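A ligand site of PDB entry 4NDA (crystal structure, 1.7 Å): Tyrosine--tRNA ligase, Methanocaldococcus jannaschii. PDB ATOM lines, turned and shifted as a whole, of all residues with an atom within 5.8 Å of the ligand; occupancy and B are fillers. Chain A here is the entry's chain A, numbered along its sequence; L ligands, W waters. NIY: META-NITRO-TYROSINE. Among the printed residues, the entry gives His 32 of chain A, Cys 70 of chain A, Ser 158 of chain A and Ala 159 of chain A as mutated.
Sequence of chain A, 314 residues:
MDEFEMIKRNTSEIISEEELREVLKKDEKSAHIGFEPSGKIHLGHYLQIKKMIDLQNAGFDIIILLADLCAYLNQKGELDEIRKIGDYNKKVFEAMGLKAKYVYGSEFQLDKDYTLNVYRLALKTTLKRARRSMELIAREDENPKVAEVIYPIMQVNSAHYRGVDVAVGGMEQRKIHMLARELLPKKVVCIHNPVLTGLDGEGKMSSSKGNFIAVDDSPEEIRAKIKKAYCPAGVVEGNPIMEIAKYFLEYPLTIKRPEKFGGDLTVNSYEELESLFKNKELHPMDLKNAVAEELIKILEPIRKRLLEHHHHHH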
ATOM      1  N   HIS A  32       0.010 -15.761 -36.575  1.00  0.00           N
ATOM      2  CA  HIS A  32       0.804 -16.587 -35.677  1.00  0.00           C
ATOM      3  C   HIS A  32      -0.042 -17.293 -34.647  1.00  0.00           C
ATOM      4  O   HIS A  32      -1.202 -16.928 -34.417  1.00  0.00           O
ATOM      5  CB  HIS A  32       1.998 -15.827 -35.054  1.00  0.00           C
ATOM      6  CG  HIS A  32       1.673 -15.069 -33.793  1.00  0.00           C
ATOM      7  ND1 HIS A  32       2.611 -14.294 -33.145  1.00  0.00           N
ATOM      8  CD2 HIS A  32       0.538 -14.975 -33.065  1.00  0.00           C
ATOM      9  CE1 HIS A  32       2.067 -13.741 -32.073  1.00  0.00           C
ATOM     10  NE2 HIS A  32       0.806 -14.146 -31.998  1.00  0.00           N
ATOM     11  N   ILE A  33       0.517 -18.341 -34.064  1.00  0.00           N
ATOM     12  CA  ILE A  33      -0.095 -18.987 -32.917  1.00  0.00           C
ATOM     13  C   ILE A  33       1.050 -19.315 -31.973  1.00  0.00           C
ATOM     14  O   ILE A  33       2.150 -19.660 -32.421  1.00  0.00           O
ATOM     15  CB  ILE A  33      -0.906 -20.254 -33.322  1.00  0.00           C
ATOM     16  CG1 ILE A  33      -1.495 -20.937 -32.077  1.00  0.00           C
ATOM     17  CG2 ILE A  33      -0.029 -21.235 -34.124  1.00  0.00           C
ATOM     18  CD1 ILE A  33      -2.517 -22.029 -32.433  1.00  0.00           C
ATOM     19  N   GLY A  34       0.818 -19.171 -30.680  1.00  0.00           N
ATOM     20  CA  GLY A  34       1.833 -19.545 -29.710  1.00  0.00           C
ATOM     21  C   GLY A  34       1.414 -20.766 -28.941  1.00  0.00           C
ATOM     22  O   GLY A  34       0.235 -20.952 -28.633  1.00  0.00           O
ATOM     23  N   PHE A  35       2.371 -21.621 -28.596  1.00  0.00           N
ATOM     24  CA  PHE A  35       2.090 -22.783 -27.750  1.00  0.00           C
ATOM     25  C   PHE A  35       3.124 -22.828 -26.658  1.00  0.00           C
ATOM     26  O   PHE A  35       4.327 -22.776 -26.956  1.00  0.00           O
ATOM     27  CB  PHE A  35       2.255 -24.112 -28.511  1.00  0.00           C
ATOM     28  CG  PHE A  35       1.303 -24.327 -29.660  1.00  0.00           C
ATOM     29  CD1 PHE A  35      -0.017 -24.709 -29.437  1.00  0.00           C
ATOM     30  CD2 PHE A  35       1.757 -24.223 -30.965  1.00  0.00           C
ATOM     31  CE1 PHE A  35      -0.891 -24.938 -30.502  1.00  0.00           C
ATOM     32  CE2 PHE A  35       0.895 -24.456 -32.051  1.00  0.00           C
ATOM     33  CZ  PHE A  35      -0.434 -24.812 -31.809  1.00  0.00           C
ATOM     34  N   GLU A  36       2.694 -22.968 -25.405  1.00  0.00           N
ATOM     35  CA  GLU A  36       3.597 -23.453 -24.377  1.00  0.00           C
ATOM     36  C   GLU A  36       4.050 -24.826 -24.834  1.00  0.00           C
ATOM     37  O   GLU A  36       3.222 -25.674 -25.156  1.00  0.00           O
ATOM     38  CB  GLU A  36       2.873 -23.585 -23.043  1.00  0.00           C
ATOM     39  CG  GLU A  36       2.394 -22.251 -22.507  1.00  0.00           C
ATOM     40  CD  GLU A  36       1.892 -22.367 -21.075  1.00  0.00           C
ATOM     41  OE1 GLU A  36       2.459 -23.187 -20.301  1.00  0.00           O
ATOM     42  OE2 GLU A  36       0.915 -21.653 -20.720  1.00  0.00           O
ATOM     43  N   LEU A  65       5.019 -19.568 -32.618  1.00  0.00           N
ATOM     44  CA  LEU A  65       5.731 -19.094 -31.439  1.00  0.00           C
ATOM     45  C   LEU A  65       5.845 -20.217 -30.412  1.00  0.00           C
ATOM     46  O   LEU A  65       4.846 -20.669 -29.845  1.00  0.00           O
ATOM     47  CB  LEU A  65       4.999 -17.882 -30.851  1.00  0.00           C
ATOM     48  CG  LEU A  65       5.529 -17.257 -29.564  1.00  0.00           C
ATOM     49  CD1 LEU A  65       7.021 -17.018 -29.744  1.00  0.00           C
ATOM     50  CD2 LEU A  65       4.803 -15.935 -29.302  1.00  0.00           C
ATOM     51  N   ALA A  67       6.448 -20.900 -27.041  1.00  0.00           N
ATOM     52  CA  ALA A  67       6.262 -19.887 -25.998  1.00  0.00           C
ATOM     53  C   ALA A  67       7.013 -20.266 -24.742  1.00  0.00           C
ATOM     54  O   ALA A  67       6.395 -20.532 -23.697  1.00  0.00           O
ATOM     55  CB  ALA A  67       4.769 -19.691 -25.693  1.00  0.00           C
ATOM     56  N   ASP A  68       8.342 -20.288 -24.829  1.00  0.00           N
ATOM     57  CA  ASP A  68       9.143 -20.759 -23.706  1.00  0.00           C
ATOM     58  C   ASP A  68       9.009 -19.872 -22.473  1.00  0.00           C
ATOM     59  O   ASP A  68       8.902 -20.378 -21.349  1.00  0.00           O
ATOM     60  CB  ASP A  68      10.621 -20.992 -24.080  1.00  0.00           C
ATOM     61  CG  ASP A  68      11.314 -19.738 -24.606  1.00  0.00           C
ATOM     62  OD1 ASP A  68      10.629 -18.795 -25.087  1.00  0.00           O
ATOM     63  OD2 ASP A  68      12.563 -19.701 -24.578  1.00  0.00           O
ATOM     64  N   LEU A  69       8.993 -18.554 -22.659  1.00  0.00           N
ATOM     65  CA  LEU A  69       8.982 -17.655 -21.508  1.00  0.00           C
ATOM     66  C   LEU A  69       7.603 -17.642 -20.840  1.00  0.00           C
ATOM     67  O   LEU A  69       7.522 -17.607 -19.624  1.00  0.00           O
ATOM     68  CB  LEU A  69       9.431 -16.243 -21.901  1.00  0.00           C
ATOM     69  CG  LEU A  69       9.511 -15.255 -20.745  1.00  0.00           C
ATOM     70  CD1 LEU A  69      10.596 -15.712 -19.761  1.00  0.00           C
ATOM     71  CD2 LEU A  69       9.815 -13.849 -21.274  1.00  0.00           C
ATOM     72  N   CYS A  70       6.536 -17.700 -21.619  1.00  0.00           N
ATOM     73  CA  CYS A  70       5.201 -17.845 -21.022  1.00  0.00           C
ATOM     74  C   CYS A  70       5.078 -19.172 -20.272  1.00  0.00           C
ATOM     75  O   CYS A  70       4.524 -19.231 -19.162  1.00  0.00           O
ATOM     76  CB  CYS A  70       4.091 -17.728 -22.090  1.00  0.00           C
ATOM     77  SG  CYS A  70       3.493 -16.002 -22.306  1.00  0.00           S
ATOM     78  N   GLY A 105       9.842 -17.400 -27.814  1.00  0.00           N
ATOM     79  CA  GLY A 105       9.422 -16.158 -27.183  1.00  0.00           C
ATOM     80  C   GLY A 105      10.611 -15.413 -26.609  1.00  0.00           C
ATOM     81  O   GLY A 105      10.778 -14.214 -26.816  1.00  0.00           O
ATOM     82  N   GLN A 109      11.369 -11.466 -26.165  1.00  0.00           N
ATOM     83  CA  GLN A 109      10.499 -11.005 -25.086  1.00  0.00           C
ATOM     84  C   GLN A 109      11.245 -10.450 -23.872  1.00  0.00           C
ATOM     85  O   GLN A 109      10.635  -9.991 -22.909  1.00  0.00           O
ATOM     86  CB  GLN A 109       9.566 -12.140 -24.645  1.00  0.00           C
ATOM     87  CG  GLN A 109       8.469 -12.405 -25.665  1.00  0.00           C
ATOM     88  CD  GLN A 109       7.621 -13.619 -25.314  1.00  0.00           C
ATOM     89  OE1 GLN A 109       8.121 -14.599 -24.760  1.00  0.00           O
ATOM     90  NE2 GLN A 109       6.333 -13.546 -25.632  1.00  0.00           N
ATOM     91  N   TYR A 114      10.688  -4.389 -25.365  1.00  0.00           N
ATOM     92  CA  TYR A 114       9.599  -5.295 -25.085  1.00  0.00           C
ATOM     93  C   TYR A 114       9.171  -5.141 -23.618  1.00  0.00           C
ATOM     94  O   TYR A 114       7.984  -5.012 -23.295  1.00  0.00           O
ATOM     95  CB  TYR A 114      10.006  -6.740 -25.339  1.00  0.00           C
ATOM     96  CG  TYR A 114       8.840  -7.678 -25.483  1.00  0.00           C
ATOM     97  CD1 TYR A 114       8.142  -8.142 -24.383  1.00  0.00           C
ATOM     98  CD2 TYR A 114       8.430  -8.094 -26.749  1.00  0.00           C
ATOM     99  CE1 TYR A 114       7.055  -8.989 -24.523  1.00  0.00           C
ATOM    100  CE2 TYR A 114       7.345  -8.939 -26.899  1.00  0.00           C
ATOM    101  CZ  TYR A 114       6.658  -9.385 -25.790  1.00  0.00           C
ATOM    102  OH  TYR A 114       5.583 -10.239 -25.941  1.00  0.00           O
ATOM    103  N   ILE A 137      -6.093 -21.174 -18.459  1.00  0.00           N
ATOM    104  CA  ILE A 137      -4.715 -21.334 -18.932  1.00  0.00           C
ATOM    105  C   ILE A 137      -3.771 -21.551 -17.767  1.00  0.00           C
ATOM    106  O   ILE A 137      -2.845 -22.368 -17.835  1.00  0.00           O
ATOM    107  CB  ILE A 137      -4.264 -20.059 -19.676  1.00  0.00           C
ATOM    108  CG1 ILE A 137      -4.961 -19.965 -21.036  1.00  0.00           C
ATOM    109  CG2 ILE A 137      -2.752 -20.103 -19.933  1.00  0.00           C
ATOM    110  CD1 ILE A 137      -4.839 -18.604 -21.677  1.00  0.00           C
ATOM    111  N   TYR A 151       1.961 -13.105 -17.289  1.00  0.00           N
ATOM    112  CA  TYR A 151       1.748 -13.939 -18.466  1.00  0.00           C
ATOM    113  C   TYR A 151       0.789 -13.321 -19.500  1.00  0.00           C
ATOM    114  O   TYR A 151       1.132 -13.250 -20.696  1.00  0.00           O
ATOM    115  CB  TYR A 151       1.255 -15.307 -18.011  1.00  0.00           C
ATOM    116  CG  TYR A 151       1.012 -16.365 -19.070  1.00  0.00           C
ATOM    117  CD1 TYR A 151       0.060 -16.182 -20.054  1.00  0.00           C
ATOM    118  CD2 TYR A 151       1.661 -17.595 -18.989  1.00  0.00           C
ATOM    119  CE1 TYR A 151      -0.203 -17.203 -21.006  1.00  0.00           C
ATOM    120  CE2 TYR A 151       1.403 -18.618 -19.909  1.00  0.00           C
ATOM    121  CZ  TYR A 151       0.478 -18.414 -20.924  1.00  0.00           C
ATOM    122  OH  TYR A 151       0.227 -19.445 -21.824  1.00  0.00           O
ATOM    123  N   MET A 154       2.354 -10.368 -21.287  1.00  0.00           N
ATOM    124  CA  MET A 154       3.414 -10.866 -22.153  1.00  0.00           C
ATOM    125  C   MET A 154       2.813 -11.266 -23.490  1.00  0.00           C
ATOM    126  O   MET A 154       3.330 -10.932 -24.561  1.00  0.00           O
ATOM    127  CB  MET A 154       4.085 -12.081 -21.481  1.00  0.00           C
ATOM    128  CG  MET A 154       5.192 -12.738 -22.299  1.00  0.00           C
ATOM    129  SD  MET A 154       6.653 -11.688 -22.505  1.00  0.00           S
ATOM    130  CE  MET A 154       6.904 -11.092 -20.835  1.00  0.00           C
ATOM    131  N   GLN A 155       1.687 -11.958 -23.441  1.00  0.00           N
ATOM    132  CA  GLN A 155       1.030 -12.442 -24.657  1.00  0.00           C
ATOM    133  C   GLN A 155       0.365 -11.313 -25.444  1.00  0.00           C
ATOM    134  O   GLN A 155       0.394 -11.295 -26.682  1.00  0.00           O
ATOM    135  CB  GLN A 155       0.005 -13.532 -24.324  1.00  0.00           C
ATOM    136  CG  GLN A 155      -0.698 -14.137 -25.526  1.00  0.00           C
ATOM    137  CD  GLN A 155      -1.421 -15.430 -25.181  1.00  0.00           C
ATOM    138  OE1 GLN A 155      -1.078 -16.107 -24.212  1.00  0.00           O
ATOM    139  NE2 GLN A 155      -2.447 -15.774 -25.970  1.00  0.00           N
ATOM    140  N   VAL A 156      -0.229 -10.358 -24.730  1.00  0.00           N
ATOM    141  CA  VAL A 156      -0.732  -9.161 -25.379  1.00  0.00           C
ATOM    142  C   VAL A 156       0.347  -8.429 -26.165  1.00  0.00           C
ATOM    143  O   VAL A 156       0.149  -8.072 -27.332  1.00  0.00           O
ATOM    144  CB  VAL A 156      -1.408  -8.205 -24.367  1.00  0.00           C
ATOM    145  CG1 VAL A 156      -1.688  -6.842 -25.035  1.00  0.00           C
ATOM    146  CG2 VAL A 156      -2.701  -8.806 -23.841  1.00  0.00           C
ATOM    147  N   SER A 158       3.109  -9.604 -27.396  1.00  0.00           N
ATOM    148  CA  SER A 158       3.652 -10.486 -28.415  1.00  0.00           C
ATOM    149  C   SER A 158       3.038 -10.190 -29.784  1.00  0.00           C
ATOM    150  O   SER A 158       3.748 -10.053 -30.785  1.00  0.00           O
ATOM    151  CB  SER A 158       3.389 -11.936 -28.003  1.00  0.00           C
ATOM    152  OG  SER A 158       3.850 -12.843 -28.970  1.00  0.00           O
ATOM    153  N   ALA A 159       1.713 -10.110 -29.827  1.00  0.00           N
ATOM    154  CA  ALA A 159       1.020  -9.833 -31.076  1.00  0.00           C
ATOM    155  C   ALA A 159       1.445  -8.467 -31.630  1.00  0.00           C
ATOM    156  O   ALA A 159       1.793  -8.322 -32.799  1.00  0.00           O
ATOM    157  CB  ALA A 159      -0.477  -9.891 -30.864  1.00  0.00           C
ATOM    158  N   GLU A 172      -9.768 -20.919 -25.227  1.00  0.00           N
ATOM    159  CA  GLU A 172      -9.264 -20.585 -23.898  1.00  0.00           C
ATOM    160  C   GLU A 172      -8.413 -19.310 -23.926  1.00  0.00           C
ATOM    161  O   GLU A 172      -8.203 -18.672 -22.883  1.00  0.00           O
ATOM    162  CB  GLU A 172      -8.492 -21.768 -23.273  1.00  0.00           C
ATOM    163  CG  GLU A 172      -7.099 -21.998 -23.844  1.00  0.00           C
ATOM    164  CD  GLU A 172      -7.095 -22.666 -25.214  1.00  0.00           C
ATOM    165  OE1 GLU A 172      -6.063 -22.559 -25.921  1.00  0.00           O
ATOM    166  OE2 GLU A 172      -8.108 -23.307 -25.579  1.00  0.00           O
ATOM    167  N   GLN A 173      -7.955 -18.917 -25.115  1.00  0.00           N
ATOM    168  CA  GLN A 173      -7.164 -17.698 -25.270  1.00  0.00           C
ATOM    169  C   GLN A 173      -7.997 -16.455 -25.475  1.00  0.00           C
ATOM    170  O   GLN A 173      -7.463 -15.343 -25.617  1.00  0.00           O
ATOM    171  CB  GLN A 173      -6.239 -17.823 -26.489  1.00  0.00           C
ATOM    172  CG  GLN A 173      -5.486 -19.148 -26.574  1.00  0.00           C
ATOM    173  CD  GLN A 173      -4.491 -19.311 -25.446  1.00  0.00           C
ATOM    174  OE1 GLN A 173      -3.801 -18.358 -25.069  1.00  0.00           O
ATOM    175  NE2 GLN A 173      -4.401 -20.514 -24.894  1.00  0.00           N
ATOM    176  N   ILE A 176      -7.568 -13.208 -23.176  1.00  0.00           N
ATOM    177  CA  ILE A 176      -6.293 -12.525 -23.428  1.00  0.00           C
ATOM    178  C   ILE A 176      -6.375 -11.764 -24.752  1.00  0.00           C
ATOM    179  O   ILE A 176      -5.953 -10.617 -24.858  1.00  0.00           O
ATOM    180  CB  ILE A 176      -5.105 -13.526 -23.472  1.00  0.00           C
ATOM    181  CG1 ILE A 176      -4.750 -14.012 -22.066  1.00  0.00           C
ATOM    182  CG2 ILE A 176      -3.876 -12.861 -24.073  1.00  0.00           C
ATOM    183  CD1 ILE A 176      -3.754 -15.206 -22.052  1.00  0.00           C
ATOM    184  N   HIS A 177      -6.943 -12.392 -25.767  1.00  0.00           N
ATOM    185  CA  HIS A 177      -7.111 -11.716 -27.050  1.00  0.00           C
ATOM    186  C   HIS A 177      -8.009 -10.483 -27.012  1.00  0.00           C
ATOM    187  O   HIS A 177      -7.739  -9.497 -27.698  1.00  0.00           O
ATOM    188  CB  HIS A 177      -7.611 -12.706 -28.108  1.00  0.00           C
ATOM    189  CG  HIS A 177      -6.569 -13.681 -28.546  1.00  0.00           C
ATOM    190  ND1 HIS A 177      -6.863 -14.802 -29.281  1.00  0.00           N
ATOM    191  CD2 HIS A 177      -5.222 -13.682 -28.375  1.00  0.00           C
ATOM    192  CE1 HIS A 177      -5.743 -15.468 -29.529  1.00  0.00           C
ATOM    193  NE2 HIS A 177      -4.742 -14.807 -28.986  1.00  0.00           N
HETATM  194  N   NIY L   1      -1.191 -18.866 -24.212  1.00  0.00           N
HETATM  195  CA  NIY L   1      -0.624 -19.849 -25.048  1.00  0.00           C
HETATM  196  C   NIY L   1      -0.902 -21.213 -24.607  1.00  0.00           C
HETATM  197  O   NIY L   1      -0.256 -22.205 -25.056  1.00  0.00           O
HETATM  198  CB  NIY L   1       0.752 -19.577 -25.473  1.00  0.00           C
HETATM  199  CG  NIY L   1       1.039 -18.283 -26.186  1.00  0.00           C
HETATM  200  CD1 NIY L   1       2.103 -17.485 -25.766  1.00  0.00           C
HETATM  201  CD2 NIY L   1       0.256 -17.882 -27.267  1.00  0.00           C
HETATM  202  CE1 NIY L   1       2.380 -16.297 -26.421  1.00  0.00           C
HETATM  203  CE2 NIY L   1       0.523 -16.694 -27.923  1.00  0.00           C
HETATM  204  CZ  NIY L   1       1.596 -15.905 -27.505  1.00  0.00           C
HETATM  205  OH  NIY L   1       1.844 -14.724 -28.168  1.00  0.00           O
HETATM  206  NN  NIY L   1       3.487 -15.517 -25.957  1.00  0.00           N
HETATM  207  O1  NIY L   1       3.557 -14.304 -26.187  1.00  0.00           O
HETATM  208  O2  NIY L   1       4.415 -16.095 -25.259  1.00  0.00           O
HETATM  209  OXT NIY L   1      -1.810 -21.401 -23.757  1.00  0.00           O
HETATM  210  O   HOH W   1      -1.108 -24.569 -25.431  1.00  0.00           O
HETATM  211  O   HOH W   2      -1.956 -18.015 -29.975  1.00  0.00           O
HETATM  212  O   HOH W   3      -2.101 -15.292 -29.376  1.00  0.00           O
HETATM  213  O   HOH W   4      -2.522 -23.491 -22.415  1.00  0.00           O
HETATM  214  O   HOH W   5       6.843 -16.942 -24.524  1.00  0.00           O
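Water W5 lies within hydrogen-bond range of an oxygen (O2) of the ligand (2.7 Å), the side-chain amide oxygen (OE1) of Gln 109 (2.7 Å), the backbone NH (N) of Cys 70 (3.0 Å) and the backbone NH (N) of Leu 69 (3.3 Å). Water W3 bridges a ring nitrogen (NE2) of His 177 (2.7 Å) and the side-chain amide nitrogen (NE2) of Gln 155 (3.5 Å).
OE1 of Gln 173 sits at hydrogen-bond distance from NE2 of Gln 155, 3.1 Å away. OE1 of Glu 172 is in hydrogen-bond range of NE2 of Gln 173 (2.8 Å). The side-chain carboxylate (OE2) of Glu 36 is in hydrogen-bond range of the side-chain hydroxyl (OH) of Tyr 151, at 2.6 Å. The backbone NH (N) of Ser 158 sits at hydrogen-bond distance from the side-chain hydroxyl (OH) of Tyr 114 (2.9 Å). The side-chain amide nitrogen of Gln 109 sits close to the side-chain sulfur of Met 154 (3.7 Å). OE1 of Gln 109 lies close to O of Gly 105 (3.4 Å). The backbone NH of Leu 65 sits at hydrogen-bond distance from the backbone carbonyl oxygen of Ile 33 (2.9 Å). The backbone NH (N) of Ala 67 sits at hydrogen-bond distance from the backbone carbonyl oxygen (O) of Phe 35 (2.8 Å).
OE1 of Gln 155 sits at hydrogen-bond distance from N of the ligand (2.8 Å). The side-chain amide oxygen of Gln 173 sits at hydrogen-bond distance from a nitrogen (N) of the ligand. The side-chain hydroxyl (OH) of Tyr 151 is in hydrogen-bond range of a nitrogen (N) of the ligand, at 2.8 Å. The side-chain hydroxyl of Ser 158 is in hydrogen-bond range of an oxygen (OH) of the ligand. The side-chain amide nitrogen (NE2) of Gln 109 is in hydrogen-bond range of an oxygen (O1) of the ligand (2.9 Å). N of Glu 36 sits at hydrogen-bond distance from O of the ligand (3.1 Å). The side-chain sulfur of Cys 70 lies within hydrogen-bond range of an oxygen (O2) of the ligand.
Residues that only touch the ligand: Gly 34, Phe 35, Leu 65, Ala 67 and Met 154. Hydrophobic or aromatic side chains that line the ligand: Leu 65, Ala 67 and Tyr 151. Of the 24 residues printed, 12 come within 4 Å of the ligand. The nearest printed residue that does not touch the ligand is His 32 (4.01 Å).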
